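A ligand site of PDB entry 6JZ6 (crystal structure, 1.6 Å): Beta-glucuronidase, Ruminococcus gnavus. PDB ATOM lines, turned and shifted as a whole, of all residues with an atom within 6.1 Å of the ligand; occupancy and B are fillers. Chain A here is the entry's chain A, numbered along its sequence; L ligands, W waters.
O3 of the ligand is in salt-bridge range of NZ of Lys 576, 2.8 Å away.
The guanidinium group (NH2) of Arg 570 is in salt-bridge range of an oxygen (O4) of the ligand.
ND2 of Asn 574 is in hydrogen-bond range of O3 of the ligand, at 3.1 Å.
O2 of the ligand is in hydrogen-bond range of OD2 of Asp 167 (2.9 Å).
OE1 of Glu 512 lies within salt-bridge range of N1 of the ligand (2.7 Å).
The side-chain carboxylate (OE2) of Glu 418 is in salt-bridge range of a nitrogen (N1) of the ligand (2.6 Å).
An oxygen (O4) of the ligand sits at hydrogen-bond distance from the side-chain hydroxyl (OH) of Tyr 478 (2.7 Å).
O2 of the ligand lies within hydrogen-bond range of NE1 of Trp 557, at 3.0 Å.
NE2 of His 335 is in hydrogen-bond range of O1 of the ligand, at 2.7 Å.
ND2 of Asn 472 lies within hydrogen-bond range of OE2 of Glu 512, 3.2 Å away.
The side-chain carboxylate of Asp 167 lies within hydrogen-bond range of the side-chain amide nitrogen of Asn 574, 3.0 Å away.
N of Asn 574 lies within hydrogen-bond range of O of Phe 562 (2.8 Å).
The backbone NH (N) of Lys 576 lies within hydrogen-bond range of the side-chain amide oxygen (OD1) of Asn 574 (2.9 Å).
OD1 of Asn 417 sits at hydrogen-bond distance from ND2 of Asn 472.
NH2 of Arg 570 is in salt-bridge range of OD2 of Asp 167, 2.8 Å away.
OD2 of Asp 516 is in salt-bridge range of NZ of Lys 576 (2.7 Å).
The side-chain hydroxyl (OH) of Tyr 478 sits at hydrogen-bond distance from the guanidinium group (NH2) of Arg 570, 3.1 Å away.
Residues that only touch the ligand: Asn 417 (3.7 Å), Tyr 474 (3.3 Å) and Phe 562 (3.8 Å).
Hydrophobic or aromatic side chains that line the ligand: His 335, Tyr 474, Tyr 478, Trp 557 and Phe 562.
Within 4 Å of the ligand: Asp 167, His 335, Asn 417, Glu 418, Tyr 474, Tyr 478, Glu 512, Trp 557, Phe 562, Arg 570, Asn 574 and Lys 576.
The nearest printed residue that does not touch the ligand is Glu 452 (4.2 Å).
Water W1 lies within hydrogen-bond range of an oxygen (O1) of the ligand (2.6 Å), a ring nitrogen (NE2) of His 301 (2.9 Å) and the backbone carbonyl oxygen of Asp 167 (3.2 Å).
Water W2 lies within hydrogen-bond range of an oxygen (O1) of the ligand (2.7 Å) and the backbone NH (N) of Asp 167 (2.9 Å).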
ATOM      1  N   PHE A 166     -16.815   4.200  10.559  1.00  0.00           N
ATOM      2  CA  PHE A 166     -15.417   3.784  10.593  1.00  0.00           C
ATOM      3  C   PHE A 166     -15.298   2.282  10.342  1.00  0.00           C
ATOM      4  O   PHE A 166     -16.262   1.538  10.554  1.00  0.00           O
ATOM      5  CB  PHE A 166     -14.772   4.154  11.937  1.00  0.00           C
ATOM      6  CG  PHE A 166     -15.607   3.765  13.122  1.00  0.00           C
ATOM      7  CD1 PHE A 166     -15.525   2.479  13.661  1.00  0.00           C
ATOM      8  CD2 PHE A 166     -16.475   4.688  13.698  1.00  0.00           C
ATOM      9  CE1 PHE A 166     -16.298   2.121  14.751  1.00  0.00           C
ATOM     10  CE2 PHE A 166     -17.259   4.334  14.794  1.00  0.00           C
ATOM     11  CZ  PHE A 166     -17.169   3.046  15.319  1.00  0.00           C
ATOM     12  N   ASP A 167     -14.117   1.836   9.923  1.00  0.00           N
ATOM     13  CA  ASP A 167     -13.925   0.456   9.514  1.00  0.00           C
ATOM     14  C   ASP A 167     -13.394  -0.476  10.612  1.00  0.00           C
ATOM     15  O   ASP A 167     -12.512  -1.299  10.347  1.00  0.00           O
ATOM     16  CB  ASP A 167     -13.008   0.384   8.287  1.00  0.00           C
ATOM     17  CG  ASP A 167     -12.936  -1.007   7.697  1.00  0.00           C
ATOM     18  OD1 ASP A 167     -13.959  -1.711   7.709  1.00  0.00           O
ATOM     19  OD2 ASP A 167     -11.848  -1.390   7.202  1.00  0.00           O
ATOM     20  N   PHE A 168     -13.925  -0.368  11.829  1.00  0.00           N
ATOM     21  CA  PHE A 168     -13.590  -1.367  12.837  1.00  0.00           C
ATOM     22  C   PHE A 168     -14.820  -1.702  13.636  1.00  0.00           C
ATOM     23  O   PHE A 168     -15.762  -0.903  13.714  1.00  0.00           O
ATOM     24  CB  PHE A 168     -12.419  -0.919  13.742  1.00  0.00           C
ATOM     25  CG  PHE A 168     -12.522   0.482  14.315  1.00  0.00           C
ATOM     26  CD1 PHE A 168     -12.997   0.687  15.609  1.00  0.00           C
ATOM     27  CD2 PHE A 168     -12.049   1.581  13.598  1.00  0.00           C
ATOM     28  CE1 PHE A 168     -13.058   1.960  16.166  1.00  0.00           C
ATOM     29  CE2 PHE A 168     -12.105   2.866  14.157  1.00  0.00           C
ATOM     30  CZ  PHE A 168     -12.605   3.045  15.441  1.00  0.00           C
ATOM     31  N   HIS A 301      -4.227  -1.972  15.850  1.00  0.00           N
ATOM     32  CA  HIS A 301      -5.539  -1.858  16.494  1.00  0.00           C
ATOM     33  C   HIS A 301      -5.375  -2.536  17.829  1.00  0.00           C
ATOM     34  O   HIS A 301      -4.462  -3.324  18.003  1.00  0.00           O
ATOM     35  CB  HIS A 301      -6.661  -2.535  15.695  1.00  0.00           C
ATOM     36  CG  HIS A 301      -7.501  -1.591  14.898  1.00  0.00           C
ATOM     37  ND1 HIS A 301      -8.311  -0.642  15.482  1.00  0.00           N
ATOM     38  CD2 HIS A 301      -7.657  -1.445  13.550  1.00  0.00           C
ATOM     39  CE1 HIS A 301      -8.921   0.053  14.540  1.00  0.00           C
ATOM     40  NE2 HIS A 301      -8.555  -0.424  13.357  1.00  0.00           N
ATOM     41  N   HIS A 335      -7.302   3.654  15.852  1.00  0.00           N
ATOM     42  CA  HIS A 335      -7.668   5.043  15.610  1.00  0.00           C
ATOM     43  C   HIS A 335      -8.210   5.611  16.919  1.00  0.00           C
ATOM     44  O   HIS A 335      -9.319   6.131  16.960  1.00  0.00           O
ATOM     45  CB  HIS A 335      -8.745   5.167  14.531  1.00  0.00           C
ATOM     46  CG  HIS A 335      -8.300   4.716  13.177  1.00  0.00           C
ATOM     47  ND1 HIS A 335      -7.270   5.337  12.489  1.00  0.00           N
ATOM     48  CD2 HIS A 335      -8.765   3.741  12.359  1.00  0.00           C
ATOM     49  CE1 HIS A 335      -7.127   4.754  11.305  1.00  0.00           C
ATOM     50  NE2 HIS A 335      -8.028   3.787  11.201  1.00  0.00           N
ATOM     51  N   VAL A 360     -12.360   9.743  13.946  1.00  0.00           N
ATOM     52  CA  VAL A 360     -12.504   8.961  12.745  1.00  0.00           C
ATOM     53  C   VAL A 360     -13.990   8.906  12.429  1.00  0.00           C
ATOM     54  O   VAL A 360     -14.821   8.884  13.351  1.00  0.00           O
ATOM     55  CB  VAL A 360     -11.891   7.546  12.944  1.00  0.00           C
ATOM     56  CG1 VAL A 360     -12.570   6.834  14.091  1.00  0.00           C
ATOM     57  CG2 VAL A 360     -11.986   6.730  11.700  1.00  0.00           C
ATOM     58  N   ASN A 417      -8.410  11.149  11.512  1.00  0.00           N
ATOM     59  CA  ASN A 417      -8.189  10.164  10.455  1.00  0.00           C
ATOM     60  C   ASN A 417      -9.286  10.276   9.413  1.00  0.00           C
ATOM     61  O   ASN A 417     -10.439   9.964   9.678  1.00  0.00           O
ATOM     62  CB  ASN A 417      -8.150   8.736  11.021  1.00  0.00           C
ATOM     63  CG  ASN A 417      -7.813   7.704   9.945  1.00  0.00           C
ATOM     64  OD1 ASN A 417      -6.647   7.509   9.594  1.00  0.00           O
ATOM     65  ND2 ASN A 417      -8.833   7.053   9.407  1.00  0.00           N
ATOM     66  N   GLU A 418      -8.908  10.752   8.219  1.00  0.00           N
ATOM     67  CA  GLU A 418      -9.803  10.824   7.059  1.00  0.00           C
ATOM     68  C   GLU A 418     -11.094  11.616   7.255  1.00  0.00           C
ATOM     69  O   GLU A 418     -12.174  11.140   6.915  1.00  0.00           O
ATOM     70  CB  GLU A 418     -10.133   9.402   6.601  1.00  0.00           C
ATOM     71  CG  GLU A 418      -8.881   8.599   6.280  1.00  0.00           C
ATOM     72  CD  GLU A 418      -9.175   7.147   5.910  1.00  0.00           C
ATOM     73  OE1 GLU A 418     -10.342   6.709   5.992  1.00  0.00           O
ATOM     74  OE2 GLU A 418      -8.220   6.447   5.532  1.00  0.00           O
ATOM     75  N   GLU A 452      -7.282  11.245   3.756  1.00  0.00           N
ATOM     76  CA  GLU A 452      -7.737  10.327   2.727  1.00  0.00           C
ATOM     77  C   GLU A 452      -7.411  10.916   1.354  1.00  0.00           C
ATOM     78  O   GLU A 452      -6.867  12.020   1.266  1.00  0.00           O
ATOM     79  CB  GLU A 452      -9.239  10.078   2.839  1.00  0.00           C
ATOM     80  CG  GLU A 452      -9.700   8.740   2.282  1.00  0.00           C
ATOM     81  CD  GLU A 452     -11.074   8.809   1.657  1.00  0.00           C
ATOM     82  OE1 GLU A 452     -11.975   8.082   2.097  1.00  0.00           O
ATOM     83  OE2 GLU A 452     -11.247   9.604   0.705  1.00  0.00           O
ATOM     84  N   LYS A 453      -7.730  10.182   0.297  1.00  0.00           N
ATOM     85  CA  LYS A 453      -7.452  10.642  -1.054  1.00  0.00           C
ATOM     86  C   LYS A 453      -8.360  11.803  -1.478  1.00  0.00           C
ATOM     87  O   LYS A 453      -7.971  12.631  -2.287  1.00  0.00           O
ATOM     88  CB  LYS A 453      -7.592   9.471  -2.037  1.00  0.00           C
ATOM     89  CG  LYS A 453      -7.266   9.817  -3.481  1.00  0.00           C
ATOM     90  CD  LYS A 453      -7.426   8.595  -4.371  1.00  0.00           C
ATOM     91  CE  LYS A 453      -7.464   8.987  -5.843  1.00  0.00           C
ATOM     92  NZ  LYS A 453      -8.773   9.590  -6.212  1.00  0.00           N
ATOM     93  N   ASN A 472      -2.992   8.571   3.745  1.00  0.00           N
ATOM     94  CA  ASN A 472      -3.496   7.208   3.581  1.00  0.00           C
ATOM     95  C   ASN A 472      -3.777   6.997   2.097  1.00  0.00           C
ATOM     96  O   ASN A 472      -4.636   7.671   1.544  1.00  0.00           O
ATOM     97  CB  ASN A 472      -4.784   7.004   4.380  1.00  0.00           C
ATOM     98  CG  ASN A 472      -4.590   7.190   5.881  1.00  0.00           C
ATOM     99  OD1 ASN A 472      -3.464   7.250   6.379  1.00  0.00           O
ATOM    100  ND2 ASN A 472      -5.700   7.251   6.605  1.00  0.00           N
ATOM    101  N   TYR A 474      -4.158   4.134  -1.330  1.00  0.00           N
ATOM    102  CA  TYR A 474      -4.379   2.754  -1.728  1.00  0.00           C
ATOM    103  C   TYR A 474      -4.347   2.635  -3.242  1.00  0.00           C
ATOM    104  O   TYR A 474      -5.224   2.021  -3.860  1.00  0.00           O
ATOM    105  CB  TYR A 474      -5.704   2.251  -1.151  1.00  0.00           C
ATOM    106  CG  TYR A 474      -5.640   2.073   0.348  1.00  0.00           C
ATOM    107  CD1 TYR A 474      -5.318   0.842   0.910  1.00  0.00           C
ATOM    108  CD2 TYR A 474      -5.926   3.135   1.197  1.00  0.00           C
ATOM    109  CE1 TYR A 474      -5.261   0.677   2.280  1.00  0.00           C
ATOM    110  CE2 TYR A 474      -5.859   2.980   2.578  1.00  0.00           C
ATOM    111  CZ  TYR A 474      -5.542   1.741   3.105  1.00  0.00           C
ATOM    112  OH  TYR A 474      -5.479   1.559   4.467  1.00  0.00           O
ATOM    113  N   TYR A 478      -7.785   0.171  -3.764  1.00  0.00           N
ATOM    114  CA  TYR A 478      -9.079   0.794  -4.042  1.00  0.00           C
ATOM    115  C   TYR A 478      -9.064   1.558  -5.364  1.00  0.00           C
ATOM    116  O   TYR A 478     -10.106   1.743  -5.984  1.00  0.00           O
ATOM    117  CB  TYR A 478      -9.477   1.732  -2.883  1.00  0.00           C
ATOM    118  CG  TYR A 478      -9.792   1.022  -1.590  1.00  0.00           C
ATOM    119  CD1 TYR A 478     -10.786   0.053  -1.532  1.00  0.00           C
ATOM    120  CD2 TYR A 478      -9.122   1.334  -0.423  1.00  0.00           C
ATOM    121  CE1 TYR A 478     -11.089  -0.600  -0.350  1.00  0.00           C
ATOM    122  CE2 TYR A 478      -9.420   0.684   0.782  1.00  0.00           C
ATOM    123  CZ  TYR A 478     -10.408  -0.274   0.795  1.00  0.00           C
ATOM    124  OH  TYR A 478     -10.727  -0.926   1.962  1.00  0.00           O
ATOM    125  N   GLU A 512      -1.124   4.903   5.828  1.00  0.00           N
ATOM    126  CA  GLU A 512      -1.845   3.703   5.412  1.00  0.00           C
ATOM    127  C   GLU A 512      -1.518   3.391   3.973  1.00  0.00           C
ATOM    128  O   GLU A 512      -1.444   4.287   3.147  1.00  0.00           O
ATOM    129  CB  GLU A 512      -3.363   3.854   5.542  1.00  0.00           C
ATOM    130  CG  GLU A 512      -3.859   3.932   6.971  1.00  0.00           C
ATOM    131  CD  GLU A 512      -5.367   3.964   7.068  1.00  0.00           C
ATOM    132  OE1 GLU A 512      -6.071   3.550   6.118  1.00  0.00           O
ATOM    133  OE2 GLU A 512      -5.861   4.408   8.134  1.00  0.00           O
ATOM    134  N   ASP A 516      -6.096  -6.193   1.116  1.00  0.00           N
ATOM    135  CA  ASP A 516      -6.657  -7.358   1.813  1.00  0.00           C
ATOM    136  C   ASP A 516      -6.009  -8.605   1.262  1.00  0.00           C
ATOM    137  O   ASP A 516      -5.882  -8.765   0.047  1.00  0.00           O
ATOM    138  CB  ASP A 516      -8.171  -7.430   1.662  1.00  0.00           C
ATOM    139  CG  ASP A 516      -8.885  -6.468   2.551  1.00  0.00           C
ATOM    140  OD1 ASP A 516      -9.330  -6.898   3.652  1.00  0.00           O
ATOM    141  OD2 ASP A 516      -8.960  -5.286   2.166  1.00  0.00           O
ATOM    142  N   TRP A 557      -0.732  -0.333   6.559  1.00  0.00           N
ATOM    143  CA  TRP A 557      -2.031  -0.728   7.071  1.00  0.00           C
ATOM    144  C   TRP A 557      -2.243  -2.182   6.712  1.00  0.00           C
ATOM    145  O   TRP A 557      -2.298  -2.502   5.517  1.00  0.00           O
ATOM    146  CB  TRP A 557      -3.135   0.121   6.440  1.00  0.00           C
ATOM    147  CG  TRP A 557      -4.413  -0.022   7.165  1.00  0.00           C
ATOM    148  CD1 TRP A 557      -5.551  -0.630   6.724  1.00  0.00           C
ATOM    149  CD2 TRP A 557      -4.690   0.422   8.504  1.00  0.00           C
ATOM    150  NE1 TRP A 557      -6.533  -0.586   7.695  1.00  0.00           N
ATOM    151  CE2 TRP A 557      -6.029   0.061   8.795  1.00  0.00           C
ATOM    152  CE3 TRP A 557      -3.939   1.119   9.473  1.00  0.00           C
ATOM    153  CZ2 TRP A 557      -6.637   0.365  10.007  1.00  0.00           C
ATOM    154  CZ3 TRP A 557      -4.544   1.414  10.681  1.00  0.00           C
ATOM    155  CH2 TRP A 557      -5.881   1.033  10.942  1.00  0.00           C
ATOM    156  N   PHE A 562      -7.889  -7.656  11.592  1.00  0.00           N
ATOM    157  CA  PHE A 562      -8.660  -7.182  12.725  1.00  0.00           C
ATOM    158  C   PHE A 562     -10.164  -7.167  12.418  1.00  0.00           C
ATOM    159  O   PHE A 562     -10.562  -7.189  11.237  1.00  0.00           O
ATOM    160  CB  PHE A 562      -8.192  -5.777  13.166  1.00  0.00           C
ATOM    161  CG  PHE A 562      -8.380  -4.708  12.110  1.00  0.00           C
ATOM    162  CD1 PHE A 562      -9.579  -4.001  12.036  1.00  0.00           C
ATOM    163  CD2 PHE A 562      -7.357  -4.381  11.235  1.00  0.00           C
ATOM    164  CE1 PHE A 562      -9.763  -3.010  11.076  1.00  0.00           C
ATOM    165  CE2 PHE A 562      -7.528  -3.389  10.281  1.00  0.00           C
ATOM    166  CZ  PHE A 562      -8.734  -2.695  10.206  1.00  0.00           C
ATOM    167  N   THR A 564     -13.987  -6.079  11.815  1.00  0.00           N
ATOM    168  CA  THR A 564     -14.822  -4.980  11.351  1.00  0.00           C
ATOM    169  C   THR A 564     -16.286  -5.383  11.475  1.00  0.00           C
ATOM    170  O   THR A 564     -16.593  -6.524  11.805  1.00  0.00           O
ATOM    171  CB  THR A 564     -14.534  -4.642   9.876  1.00  0.00           C
ATOM    172  OG1 THR A 564     -14.896  -5.752   9.049  1.00  0.00           O
ATOM    173  CG2 THR A 564     -13.062  -4.325   9.674  1.00  0.00           C
ATOM    174  N   ARG A 570     -16.058  -7.227   3.603  1.00  0.00           N
ATOM    175  CA  ARG A 570     -15.201  -7.653   4.705  1.00  0.00           C
ATOM    176  C   ARG A 570     -15.364  -9.147   4.980  1.00  0.00           C
ATOM    177  O   ARG A 570     -16.421  -9.602   5.418  1.00  0.00           O
ATOM    178  CB  ARG A 570     -15.513  -6.825   5.961  1.00  0.00           C
ATOM    179  CG  ARG A 570     -15.081  -5.355   5.851  1.00  0.00           C
ATOM    180  CD  ARG A 570     -13.548  -5.250   5.870  1.00  0.00           C
ATOM    181  NE  ARG A 570     -13.064  -3.867   5.685  1.00  0.00           N
ATOM    182  CZ  ARG A 570     -12.598  -3.384   4.537  1.00  0.00           C
ATOM    183  NH1 ARG A 570     -12.615  -4.140   3.439  1.00  0.00           N
ATOM    184  NH2 ARG A 570     -12.159  -2.131   4.474  1.00  0.00           N
ATOM    185  N   ASN A 574     -11.073  -7.196   8.478  1.00  0.00           N
ATOM    186  CA  ASN A 574     -10.186  -6.526   7.537  1.00  0.00           C
ATOM    187  C   ASN A 574      -8.921  -7.375   7.445  1.00  0.00           C
ATOM    188  O   ASN A 574      -8.314  -7.685   8.473  1.00  0.00           O
ATOM    189  CB  ASN A 574      -9.914  -5.104   8.030  1.00  0.00           C
ATOM    190  CG  ASN A 574      -8.994  -4.295   7.112  1.00  0.00           C
ATOM    191  OD1 ASN A 574      -7.874  -4.726   6.790  1.00  0.00           O
ATOM    192  ND2 ASN A 574      -9.425  -3.093   6.732  1.00  0.00           N
ATOM    193  N   LYS A 576      -6.101  -6.675   5.688  1.00  0.00           N
ATOM    194  CA  LYS A 576      -4.902  -5.970   5.231  1.00  0.00           C
ATOM    195  C   LYS A 576      -3.736  -6.167   6.182  1.00  0.00           C
ATOM    196  O   LYS A 576      -2.667  -5.601   5.980  1.00  0.00           O
ATOM    197  CB  LYS A 576      -5.189  -4.476   5.039  1.00  0.00           C
ATOM    198  CG  LYS A 576      -6.299  -4.211   4.032  1.00  0.00           C
ATOM    199  CD  LYS A 576      -6.278  -2.763   3.561  1.00  0.00           C
ATOM    200  CE  LYS A 576      -7.304  -2.547   2.447  1.00  0.00           C
ATOM    201  NZ  LYS A 576      -8.706  -2.694   2.949  1.00  0.00           N
HETATM  202  N1  LIG L   1      -8.733   3.907   6.005  1.00  0.00           N
HETATM  203  C1  LIG L   1      -9.325   4.545   1.742  1.00  0.00           C
HETATM  204  C2  LIG L   1      -9.038   3.909   7.433  1.00  0.00           C
HETATM  205  C3  LIG L   1      -8.885   2.500   8.037  1.00  0.00           C
HETATM  206  C4  LIG L   1      -9.534   1.431   7.172  1.00  0.00           C
HETATM  207  C5  LIG L   1      -8.899   1.501   5.792  1.00  0.00           C
HETATM  208  C6  LIG L   1      -9.359   0.346   4.946  1.00  0.00           C
HETATM  209  C7  LIG L   1      -9.315   2.845   5.194  1.00  0.00           C
HETATM  210  C8  LIG L   1      -8.953   3.050   3.733  1.00  0.00           C
HETATM  211  C9  LIG L   1      -9.422   4.428   3.247  1.00  0.00           C
HETATM  212  O1  LIG L   1      -9.470   2.503   9.343  1.00  0.00           O
HETATM  213  O2  LIG L   1      -9.417   0.133   7.784  1.00  0.00           O
HETATM  214  O3  LIG L   1      -8.717  -0.706   4.882  1.00  0.00           O
HETATM  215  O4  LIG L   1     -10.509   0.447   4.285  1.00  0.00           O
HETATM  216  O   HOH W   1     -10.037   0.562  11.025  1.00  0.00           O
HETATM  217  O   HOH W   2     -11.883   3.655   9.645  1.00  0.00           O
HETATM  218  O   HOH W   3     -12.914   1.747   4.962  1.00  0.00           O
